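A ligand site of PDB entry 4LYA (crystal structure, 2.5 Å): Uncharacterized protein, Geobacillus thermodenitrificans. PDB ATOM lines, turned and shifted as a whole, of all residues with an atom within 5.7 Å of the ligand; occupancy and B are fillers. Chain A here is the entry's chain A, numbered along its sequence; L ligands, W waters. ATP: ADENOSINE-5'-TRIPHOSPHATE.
The backbone carbonyl oxygen of Pro 262 sits close to a nitrogen (N1) of the ligand. Pro 36 touches the ligand (O to C2, 3.3 Å). O of Ser 82 touches O1B of the ligand, at 3.5 Å. CB of Ala 83 touches O1G of the ligand, at 3.2 Å. Tyr 85 touches the ligand. Gly 263 touches the ligand. Leu 279 touches the ligand (CD2 to N1, 3.4 Å). The nearest printed residue that does not touch the ligand is Tyr 278 (4.1 Å).
Water W2 lies within hydrogen-bond range of a nitrogen (N6) of the ligand (2.9 Å), the side-chain hydroxyl of Thr 90 (2.9 Å) and the backbone carbonyl oxygen of Gly 86 (3.1 Å). Water W5 bridges O of Pro 36 (2.6 Å) and O of Pro 262 (2.7 Å). Water W4 lies within hydrogen-bond range of OD1 of Asp 286, NH2 of Arg 37 and O2' of the ligand. Water W3 bridges O of Gly 84 (2.5 Å) and O4' of the ligand (3.4 Å).
The side-chain amino group (NZ) of Lys 87 is in hydrogen-bond range of the backbone carbonyl oxygen (O) of Ser 82 (3.0 Å). NZ of Lys 87 lies within hydrogen-bond range of O of Gly 81 (2.9 Å). The backbone NH of Ile 277 is in hydrogen-bond range of the backbone carbonyl oxygen of Gly 263 (2.8 Å). N of Gly 263 is in hydrogen-bond range of O of Tyr 85 (3.2 Å). O of Pro 36 is in hydrogen-bond range of NE2 of Gln 276 (2.9 Å). O of Leu 38 is in hydrogen-bond range of N of Leu 279 (2.6 Å). NE2 of Gln 276 is in hydrogen-bond range of O of Pro 262 (3.3 Å). The side-chain amide oxygen (OE1) of Gln 276 sits at hydrogen-bond distance from the guanidinium group (NE) of Arg 264, at 2.8 Å.
N of Thr 89 lies within hydrogen-bond range of O2A of the ligand, at 3.0 Å. The side-chain hydroxyl of Thr 89 is in hydrogen-bond range of an oxygen (O2A) of the ligand (2.4 Å). The side-chain carboxylate (OD2) of Asp 286 sits at hydrogen-bond distance from an oxygen (O3') of the ligand, at 2.4 Å. An oxygen (O1B) of the ligand sits close to the backbone NH (N) of Lys 87 (3.4 Å). The side-chain amino group (NZ) of Lys 87 is in salt-bridge range of an oxygen (O1B) of the ligand. O of Ile 277 sits at hydrogen-bond distance from N6 of the ligand (2.8 Å). An oxygen (O2B) of the ligand sits at hydrogen-bond distance from the backbone NH (N) of Ser 88 (2.8 Å). O2B of the ligand lies within hydrogen-bond range of OG of Ser 88 (2.9 Å). The backbone NH (N) of Gly 86 is in hydrogen-bond range of an oxygen (O3A) of the ligand. N of Gly 84 lies within hydrogen-bond range of O1B of the ligand. The side-chain amide nitrogen (NE2) of Gln 276 is in hydrogen-bond range of a nitrogen (N1) of the ligand (3.5 Å).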
ATOM      1  N   PRO A  36     -14.132 -23.133 -11.878  1.00  0.00           N
ATOM      2  CA  PRO A  36     -15.394 -23.633 -12.427  1.00  0.00           C
ATOM      3  C   PRO A  36     -16.424 -24.020 -11.368  1.00  0.00           C
ATOM      4  O   PRO A  36     -17.627 -23.983 -11.641  1.00  0.00           O
ATOM      5  CB  PRO A  36     -14.963 -24.869 -13.219  1.00  0.00           C
ATOM      6  CG  PRO A  36     -13.764 -25.364 -12.492  1.00  0.00           C
ATOM      7  CD  PRO A  36     -13.058 -24.141 -11.973  1.00  0.00           C
ATOM      8  N   ARG A  37     -15.970 -24.389 -10.167  1.00  0.00           N
ATOM      9  CA  ARG A  37     -16.883 -24.809  -9.106  1.00  0.00           C
ATOM     10  C   ARG A  37     -16.570 -24.158  -7.762  1.00  0.00           C
ATOM     11  O   ARG A  37     -15.448 -24.239  -7.263  1.00  0.00           O
ATOM     12  CB  ARG A  37     -16.885 -26.334  -8.965  1.00  0.00           C
ATOM     13  CG  ARG A  37     -17.190 -27.079 -10.256  1.00  0.00           C
ATOM     14  CD  ARG A  37     -17.357 -28.580 -10.027  1.00  0.00           C
ATOM     15  NE  ARG A  37     -18.734 -28.938  -9.671  1.00  0.00           N
ATOM     16  CZ  ARG A  37     -19.117 -29.318  -8.460  1.00  0.00           C
ATOM     17  NH1 ARG A  37     -18.236 -29.405  -7.474  1.00  0.00           N
ATOM     18  NH2 ARG A  37     -20.391 -29.631  -8.233  1.00  0.00           N
ATOM     19  N   LEU A  38     -17.575 -23.502  -7.183  1.00  0.00           N
ATOM     20  CA  LEU A  38     -17.439 -22.870  -5.874  1.00  0.00           C
ATOM     21  C   LEU A  38     -18.716 -23.024  -5.060  1.00  0.00           C
ATOM     22  O   LEU A  38     -19.812 -22.737  -5.548  1.00  0.00           O
ATOM     23  CB  LEU A  38     -17.105 -21.387  -6.018  1.00  0.00           C
ATOM     24  CG  LEU A  38     -15.685 -21.006  -6.461  1.00  0.00           C
ATOM     25  CD1 LEU A  38     -15.563 -19.496  -6.560  1.00  0.00           C
ATOM     26  CD2 LEU A  38     -14.655 -21.576  -5.501  1.00  0.00           C
ATOM     27  N   GLY A  81     -29.636 -17.183 -19.696  1.00  0.00           N
ATOM     28  CA  GLY A  81     -28.579 -18.038 -20.215  1.00  0.00           C
ATOM     29  C   GLY A  81     -29.117 -19.202 -21.016  1.00  0.00           C
ATOM     30  O   GLY A  81     -30.304 -19.536 -20.909  1.00  0.00           O
ATOM     31  N   SER A  82     -28.255 -19.826 -21.811  1.00  0.00           N
ATOM     32  CA  SER A  82     -28.647 -20.986 -22.594  1.00  0.00           C
ATOM     33  C   SER A  82     -28.825 -22.215 -21.697  1.00  0.00           C
ATOM     34  O   SER A  82     -28.465 -22.191 -20.519  1.00  0.00           O
ATOM     35  CB  SER A  82     -27.620 -21.278 -23.680  1.00  0.00           C
ATOM     36  OG  SER A  82     -27.600 -20.239 -24.650  1.00  0.00           O
ATOM     37  N   ALA A  83     -29.389 -23.275 -22.270  1.00  0.00           N
ATOM     38  CA  ALA A  83     -29.663 -24.506 -21.526  1.00  0.00           C
ATOM     39  C   ALA A  83     -28.378 -25.169 -21.025  1.00  0.00           C
ATOM     40  O   ALA A  83     -27.442 -25.407 -21.788  1.00  0.00           O
ATOM     41  CB  ALA A  83     -30.450 -25.468 -22.391  1.00  0.00           C
ATOM     42  N   GLY A  84     -28.338 -25.457 -19.725  1.00  0.00           N
ATOM     43  CA  GLY A  84     -27.239 -26.195 -19.130  1.00  0.00           C
ATOM     44  C   GLY A  84     -26.131 -25.323 -18.562  1.00  0.00           C
ATOM     45  O   GLY A  84     -25.068 -25.830 -18.194  1.00  0.00           O
ATOM     46  N   TYR A  85     -26.365 -24.020 -18.492  1.00  0.00           N
ATOM     47  CA  TYR A  85     -25.337 -23.107 -17.997  1.00  0.00           C
ATOM     48  C   TYR A  85     -25.654 -22.501 -16.627  1.00  0.00           C
ATOM     49  O   TYR A  85     -25.009 -21.542 -16.203  1.00  0.00           O
ATOM     50  CB  TYR A  85     -25.033 -22.027 -19.038  1.00  0.00           C
ATOM     51  CG  TYR A  85     -24.320 -22.575 -20.256  1.00  0.00           C
ATOM     52  CD1 TYR A  85     -22.970 -22.886 -20.224  1.00  0.00           C
ATOM     53  CD2 TYR A  85     -25.005 -22.812 -21.446  1.00  0.00           C
ATOM     54  CE1 TYR A  85     -22.312 -23.392 -21.324  1.00  0.00           C
ATOM     55  CE2 TYR A  85     -24.360 -23.320 -22.557  1.00  0.00           C
ATOM     56  CZ  TYR A  85     -23.012 -23.619 -22.489  1.00  0.00           C
ATOM     57  OH  TYR A  85     -22.368 -24.127 -23.601  1.00  0.00           O
ATOM     58  N   GLY A  86     -26.646 -23.073 -15.940  1.00  0.00           N
ATOM     59  CA  GLY A  86     -26.836 -22.813 -14.529  1.00  0.00           C
ATOM     60  C   GLY A  86     -27.941 -21.868 -14.096  1.00  0.00           C
ATOM     61  O   GLY A  86     -27.869 -21.297 -13.012  1.00  0.00           O
ATOM     62  N   LYS A  87     -28.984 -21.721 -14.908  1.00  0.00           N
ATOM     63  CA  LYS A  87     -30.092 -20.833 -14.570  1.00  0.00           C
ATOM     64  C   LYS A  87     -30.826 -21.274 -13.308  1.00  0.00           C
ATOM     65  O   LYS A  87     -31.004 -20.479 -12.376  1.00  0.00           O
ATOM     66  CB  LYS A  87     -31.074 -20.702 -15.735  1.00  0.00           C
ATOM     67  CG  LYS A  87     -30.563 -19.844 -16.889  1.00  0.00           C
ATOM     68  CD  LYS A  87     -31.656 -19.626 -17.922  1.00  0.00           C
ATOM     69  CE  LYS A  87     -32.138 -20.950 -18.491  1.00  0.00           C
ATOM     70  NZ  LYS A  87     -31.024 -21.723 -19.117  1.00  0.00           N
ATOM     71  N   SER A  88     -31.260 -22.527 -13.276  1.00  0.00           N
ATOM     72  CA  SER A  88     -31.995 -23.039 -12.135  1.00  0.00           C
ATOM     73  C   SER A  88     -31.090 -23.233 -10.920  1.00  0.00           C
ATOM     74  O   SER A  88     -31.546 -23.132  -9.776  1.00  0.00           O
ATOM     75  CB  SER A  88     -32.693 -24.362 -12.488  1.00  0.00           C
ATOM     76  OG  SER A  88     -31.753 -25.376 -12.771  1.00  0.00           O
ATOM     77  N   THR A  89     -29.814 -23.487 -11.167  1.00  0.00           N
ATOM     78  CA  THR A  89     -28.844 -23.671 -10.095  1.00  0.00           C
ATOM     79  C   THR A  89     -28.634 -22.373  -9.323  1.00  0.00           C
ATOM     80  O   THR A  89     -28.513 -22.380  -8.101  1.00  0.00           O
ATOM     81  CB  THR A  89     -27.491 -24.169 -10.638  1.00  0.00           C
ATOM     82  OG1 THR A  89     -27.682 -25.385 -11.370  1.00  0.00           O
ATOM     83  CG2 THR A  89     -26.508 -24.417  -9.503  1.00  0.00           C
ATOM     84  N   THR A  90     -28.614 -21.252 -10.041  1.00  0.00           N
ATOM     85  CA  THR A  90     -28.483 -19.940  -9.425  1.00  0.00           C
ATOM     86  C   THR A  90     -29.694 -19.629  -8.562  1.00  0.00           C
ATOM     87  O   THR A  90     -29.568 -19.089  -7.465  1.00  0.00           O
ATOM     88  CB  THR A  90     -28.313 -18.832 -10.492  1.00  0.00           C
ATOM     89  OG1 THR A  90     -27.135 -19.091 -11.264  1.00  0.00           O
ATOM     90  CG2 THR A  90     -28.199 -17.468  -9.838  1.00  0.00           C
ATOM     91  N   ASP A 185     -39.529 -20.392 -12.556  1.00  0.00           N
ATOM     92  CA  ASP A 185     -38.569 -21.046 -13.432  1.00  0.00           C
ATOM     93  C   ASP A 185     -39.140 -21.166 -14.831  1.00  0.00           C
ATOM     94  O   ASP A 185     -40.325 -21.469 -15.000  1.00  0.00           O
ATOM     95  CB  ASP A 185     -38.198 -22.430 -12.889  1.00  0.00           C
ATOM     96  CG  ASP A 185     -37.047 -23.057 -13.643  1.00  0.00           C
ATOM     97  OD1 ASP A 185     -36.126 -22.320 -14.051  1.00  0.00           O
ATOM     98  OD2 ASP A 185     -37.064 -24.298 -13.837  1.00  0.00           O
ATOM     99  N   THR A 220     -34.739 -18.425 -20.926  1.00  0.00           N
ATOM    100  CA  THR A 220     -33.801 -18.806 -21.972  1.00  0.00           C
ATOM    101  C   THR A 220     -33.874 -17.826 -23.136  1.00  0.00           C
ATOM    102  O   THR A 220     -32.929 -17.076 -23.390  1.00  0.00           O
ATOM    103  CB  THR A 220     -34.099 -20.224 -22.493  1.00  0.00           C
ATOM    104  OG1 THR A 220     -34.172 -21.143 -21.398  1.00  0.00           O
ATOM    105  CG2 THR A 220     -33.019 -20.678 -23.464  1.00  0.00           C
ATOM    106  N   PRO A 262     -20.594 -23.457 -16.990  1.00  0.00           N
ATOM    107  CA  PRO A 262     -21.796 -23.423 -16.150  1.00  0.00           C
ATOM    108  C   PRO A 262     -21.546 -22.710 -14.829  1.00  0.00           C
ATOM    109  O   PRO A 262     -20.682 -23.130 -14.056  1.00  0.00           O
ATOM    110  CB  PRO A 262     -22.094 -24.901 -15.907  1.00  0.00           C
ATOM    111  CG  PRO A 262     -21.479 -25.614 -17.060  1.00  0.00           C
ATOM    112  CD  PRO A 262     -20.244 -24.835 -17.390  1.00  0.00           C
ATOM    113  N   GLY A 263     -22.302 -21.648 -14.566  1.00  0.00           N
ATOM    114  CA  GLY A 263     -22.134 -20.867 -13.351  1.00  0.00           C
ATOM    115  C   GLY A 263     -21.481 -19.530 -13.610  1.00  0.00           C
ATOM    116  O   GLY A 263     -21.657 -18.588 -12.828  1.00  0.00           O
ATOM    117  N   ARG A 264     -20.737 -19.436 -14.707  1.00  0.00           N
ATOM    118  CA  ARG A 264     -20.085 -18.191 -15.095  1.00  0.00           C
ATOM    119  C   ARG A 264     -21.127 -17.217 -15.615  1.00  0.00           C
ATOM    120  O   ARG A 264     -21.917 -17.554 -16.493  1.00  0.00           O
ATOM    121  CB  ARG A 264     -19.029 -18.448 -16.156  1.00  0.00           C
ATOM    122  CG  ARG A 264     -18.177 -17.232 -16.504  1.00  0.00           C
ATOM    123  CD  ARG A 264     -17.373 -16.775 -15.307  1.00  0.00           C
ATOM    124  NE  ARG A 264     -16.660 -17.878 -14.674  1.00  0.00           N
ATOM    125  CZ  ARG A 264     -15.558 -18.442 -15.153  1.00  0.00           C
ATOM    126  NH1 ARG A 264     -15.027 -17.996 -16.293  1.00  0.00           N
ATOM    127  NH2 ARG A 264     -14.987 -19.445 -14.511  1.00  0.00           N
ATOM    128  N   GLN A 276     -18.388 -15.972 -10.933  1.00  0.00           N
ATOM    129  CA  GLN A 276     -18.723 -17.396 -10.916  1.00  0.00           C
ATOM    130  C   GLN A 276     -19.719 -17.646  -9.797  1.00  0.00           C
ATOM    131  O   GLN A 276     -19.374 -17.581  -8.617  1.00  0.00           O
ATOM    132  CB  GLN A 276     -17.465 -18.243 -10.704  1.00  0.00           C
ATOM    133  CG  GLN A 276     -17.737 -19.736 -10.646  1.00  0.00           C
ATOM    134  CD  GLN A 276     -18.278 -20.288 -11.962  1.00  0.00           C
ATOM    135  OE1 GLN A 276     -18.036 -19.719 -13.027  1.00  0.00           O
ATOM    136  NE2 GLN A 276     -18.996 -21.400 -11.881  1.00  0.00           N
ATOM    137  N   ILE A 277     -20.963 -17.926 -10.173  1.00  0.00           N
ATOM    138  CA  ILE A 277     -22.047 -18.133  -9.212  1.00  0.00           C
ATOM    139  C   ILE A 277     -21.782 -19.331  -8.309  1.00  0.00           C
ATOM    140  O   ILE A 277     -21.340 -20.376  -8.779  1.00  0.00           O
ATOM    141  CB  ILE A 277     -23.404 -18.305  -9.924  1.00  0.00           C
ATOM    142  CG1 ILE A 277     -23.706 -17.095 -10.813  1.00  0.00           C
ATOM    143  CG2 ILE A 277     -24.527 -18.489  -8.914  1.00  0.00           C
ATOM    144  CD1 ILE A 277     -23.814 -15.789 -10.059  1.00  0.00           C
ATOM    145  N   TYR A 278     -22.036 -19.160  -7.016  1.00  0.00           N
ATOM    146  CA  TYR A 278     -21.836 -20.222  -6.047  1.00  0.00           C
ATOM    147  C   TYR A 278     -22.824 -21.360  -6.207  1.00  0.00           C
ATOM    148  O   TYR A 278     -23.952 -21.160  -6.642  1.00  0.00           O
ATOM    149  CB  TYR A 278     -21.913 -19.659  -4.621  1.00  0.00           C
ATOM    150  CG  TYR A 278     -20.749 -18.785  -4.230  1.00  0.00           C
ATOM    151  CD1 TYR A 278     -19.484 -19.013  -4.754  1.00  0.00           C
ATOM    152  CD2 TYR A 278     -20.910 -17.739  -3.336  1.00  0.00           C
ATOM    153  CE1 TYR A 278     -18.415 -18.221  -4.396  1.00  0.00           C
ATOM    154  CE2 TYR A 278     -19.845 -16.935  -2.973  1.00  0.00           C
ATOM    155  CZ  TYR A 278     -18.602 -17.185  -3.506  1.00  0.00           C
ATOM    156  OH  TYR A 278     -17.532 -16.390  -3.157  1.00  0.00           O
ATOM    157  N   LEU A 279     -22.378 -22.571  -5.855  1.00  0.00           N
ATOM    158  CA  LEU A 279     -23.252 -23.742  -5.852  1.00  0.00           C
ATOM    159  C   LEU A 279     -24.113 -23.743  -4.599  1.00  0.00           C
ATOM    160  O   LEU A 279     -23.693 -23.242  -3.559  1.00  0.00           O
ATOM    161  CB  LEU A 279     -22.404 -25.017  -5.944  1.00  0.00           C
ATOM    162  CG  LEU A 279     -21.777 -25.295  -7.304  1.00  0.00           C
ATOM    163  CD1 LEU A 279     -20.728 -26.390  -7.197  1.00  0.00           C
ATOM    164  CD2 LEU A 279     -22.846 -25.682  -8.315  1.00  0.00           C
ATOM    165  N   ASP A 286     -22.989 -33.461  -8.984  1.00  0.00           N
ATOM    166  CA  ASP A 286     -24.379 -33.025  -8.889  1.00  0.00           C
ATOM    167  C   ASP A 286     -25.170 -33.730  -7.786  1.00  0.00           C
ATOM    168  O   ASP A 286     -25.832 -33.080  -6.975  1.00  0.00           O
ATOM    169  CB  ASP A 286     -25.085 -33.218 -10.233  1.00  0.00           C
ATOM    170  CG  ASP A 286     -24.617 -32.237 -11.282  1.00  0.00           C
ATOM    171  OD1 ASP A 286     -23.961 -31.241 -10.908  1.00  0.00           O
ATOM    172  OD2 ASP A 286     -24.890 -32.458 -12.484  1.00  0.00           O
HETATM  173  PG  ATP L   1     -32.056 -26.033 -18.232  1.00  0.00           P
HETATM  174  O1G ATP L   1     -31.559 -26.489 -19.575  1.00  0.00           O
HETATM  175  O2G ATP L   1     -32.930 -27.025 -17.509  1.00  0.00           O
HETATM  176  O3G ATP L   1     -32.586 -24.613 -18.217  1.00  0.00           O
HETATM  177  PB  ATP L   1     -30.258 -24.602 -16.594  1.00  0.00           P
HETATM  178  O1B ATP L   1     -30.029 -23.541 -17.644  1.00  0.00           O
HETATM  179  O2B ATP L   1     -31.193 -24.344 -15.443  1.00  0.00           O
HETATM  180  O3B ATP L   1     -30.723 -25.968 -17.325  1.00  0.00           O
HETATM  181  PA  ATP L   1     -28.747 -25.963 -14.687  1.00  0.00           P
HETATM  182  O1A ATP L   1     -29.689 -27.135 -14.879  1.00  0.00           O
HETATM  183  O2A ATP L   1     -28.887 -25.110 -13.458  1.00  0.00           O
HETATM  184  O3A ATP L   1     -28.829 -25.059 -16.016  1.00  0.00           O
HETATM  185  O5' ATP L   1     -27.242 -26.542 -14.765  1.00  0.00           O
HETATM  186  C5' ATP L   1     -27.020 -27.891 -15.138  1.00  0.00           C
HETATM  187  C4' ATP L   1     -25.605 -28.320 -14.773  1.00  0.00           C
HETATM  188  O4' ATP L   1     -24.724 -27.198 -14.814  1.00  0.00           O
HETATM  189  C3' ATP L   1     -25.550 -28.879 -13.366  1.00  0.00           C
HETATM  190  O3' ATP L   1     -25.519 -30.304 -13.411  1.00  0.00           O
HETATM  191  C2' ATP L   1     -24.274 -28.333 -12.769  1.00  0.00           C
HETATM  192  O2' ATP L   1     -23.297 -29.368 -12.665  1.00  0.00           O
HETATM  193  C1' ATP L   1     -23.785 -27.254 -13.729  1.00  0.00           C
HETATM  194  N9  ATP L   1     -23.779 -25.954 -13.016  1.00  0.00           N
HETATM  195  C8  ATP L   1     -24.798 -25.080 -12.977  1.00  0.00           C
HETATM  196  N7  ATP L   1     -24.483 -23.987 -12.230  1.00  0.00           N
HETATM  197  C5  ATP L   1     -23.232 -24.162 -11.771  1.00  0.00           C
HETATM  198  C6  ATP L   1     -22.281 -23.399 -10.928  1.00  0.00           C
HETATM  199  N6  ATP L   1     -22.627 -22.196 -10.410  1.00  0.00           N
HETATM  200  N1  ATP L   1     -21.064 -23.945 -10.686  1.00  0.00           N
HETATM  201  C2  ATP L   1     -20.714 -25.140 -11.201  1.00  0.00           C
HETATM  202  N3  ATP L   1     -21.516 -25.885 -11.969  1.00  0.00           N
HETATM  203  C4  ATP L   1     -22.767 -25.469 -12.290  1.00  0.00           C
HETATM  204  O   HOH W   1     -19.364 -22.544  -9.030  1.00  0.00           O
HETATM  205  O   HOH W   2     -25.184 -21.249 -11.384  1.00  0.00           O
HETATM  206  O   HOH W   3     -24.344 -28.259 -18.039  1.00  0.00           O
HETATM  207  O   HOH W   4     -23.129 -29.657  -9.281  1.00  0.00           O
HETATM  208  O   HOH W   5     -18.621 -24.849 -13.859  1.00  0.00           O
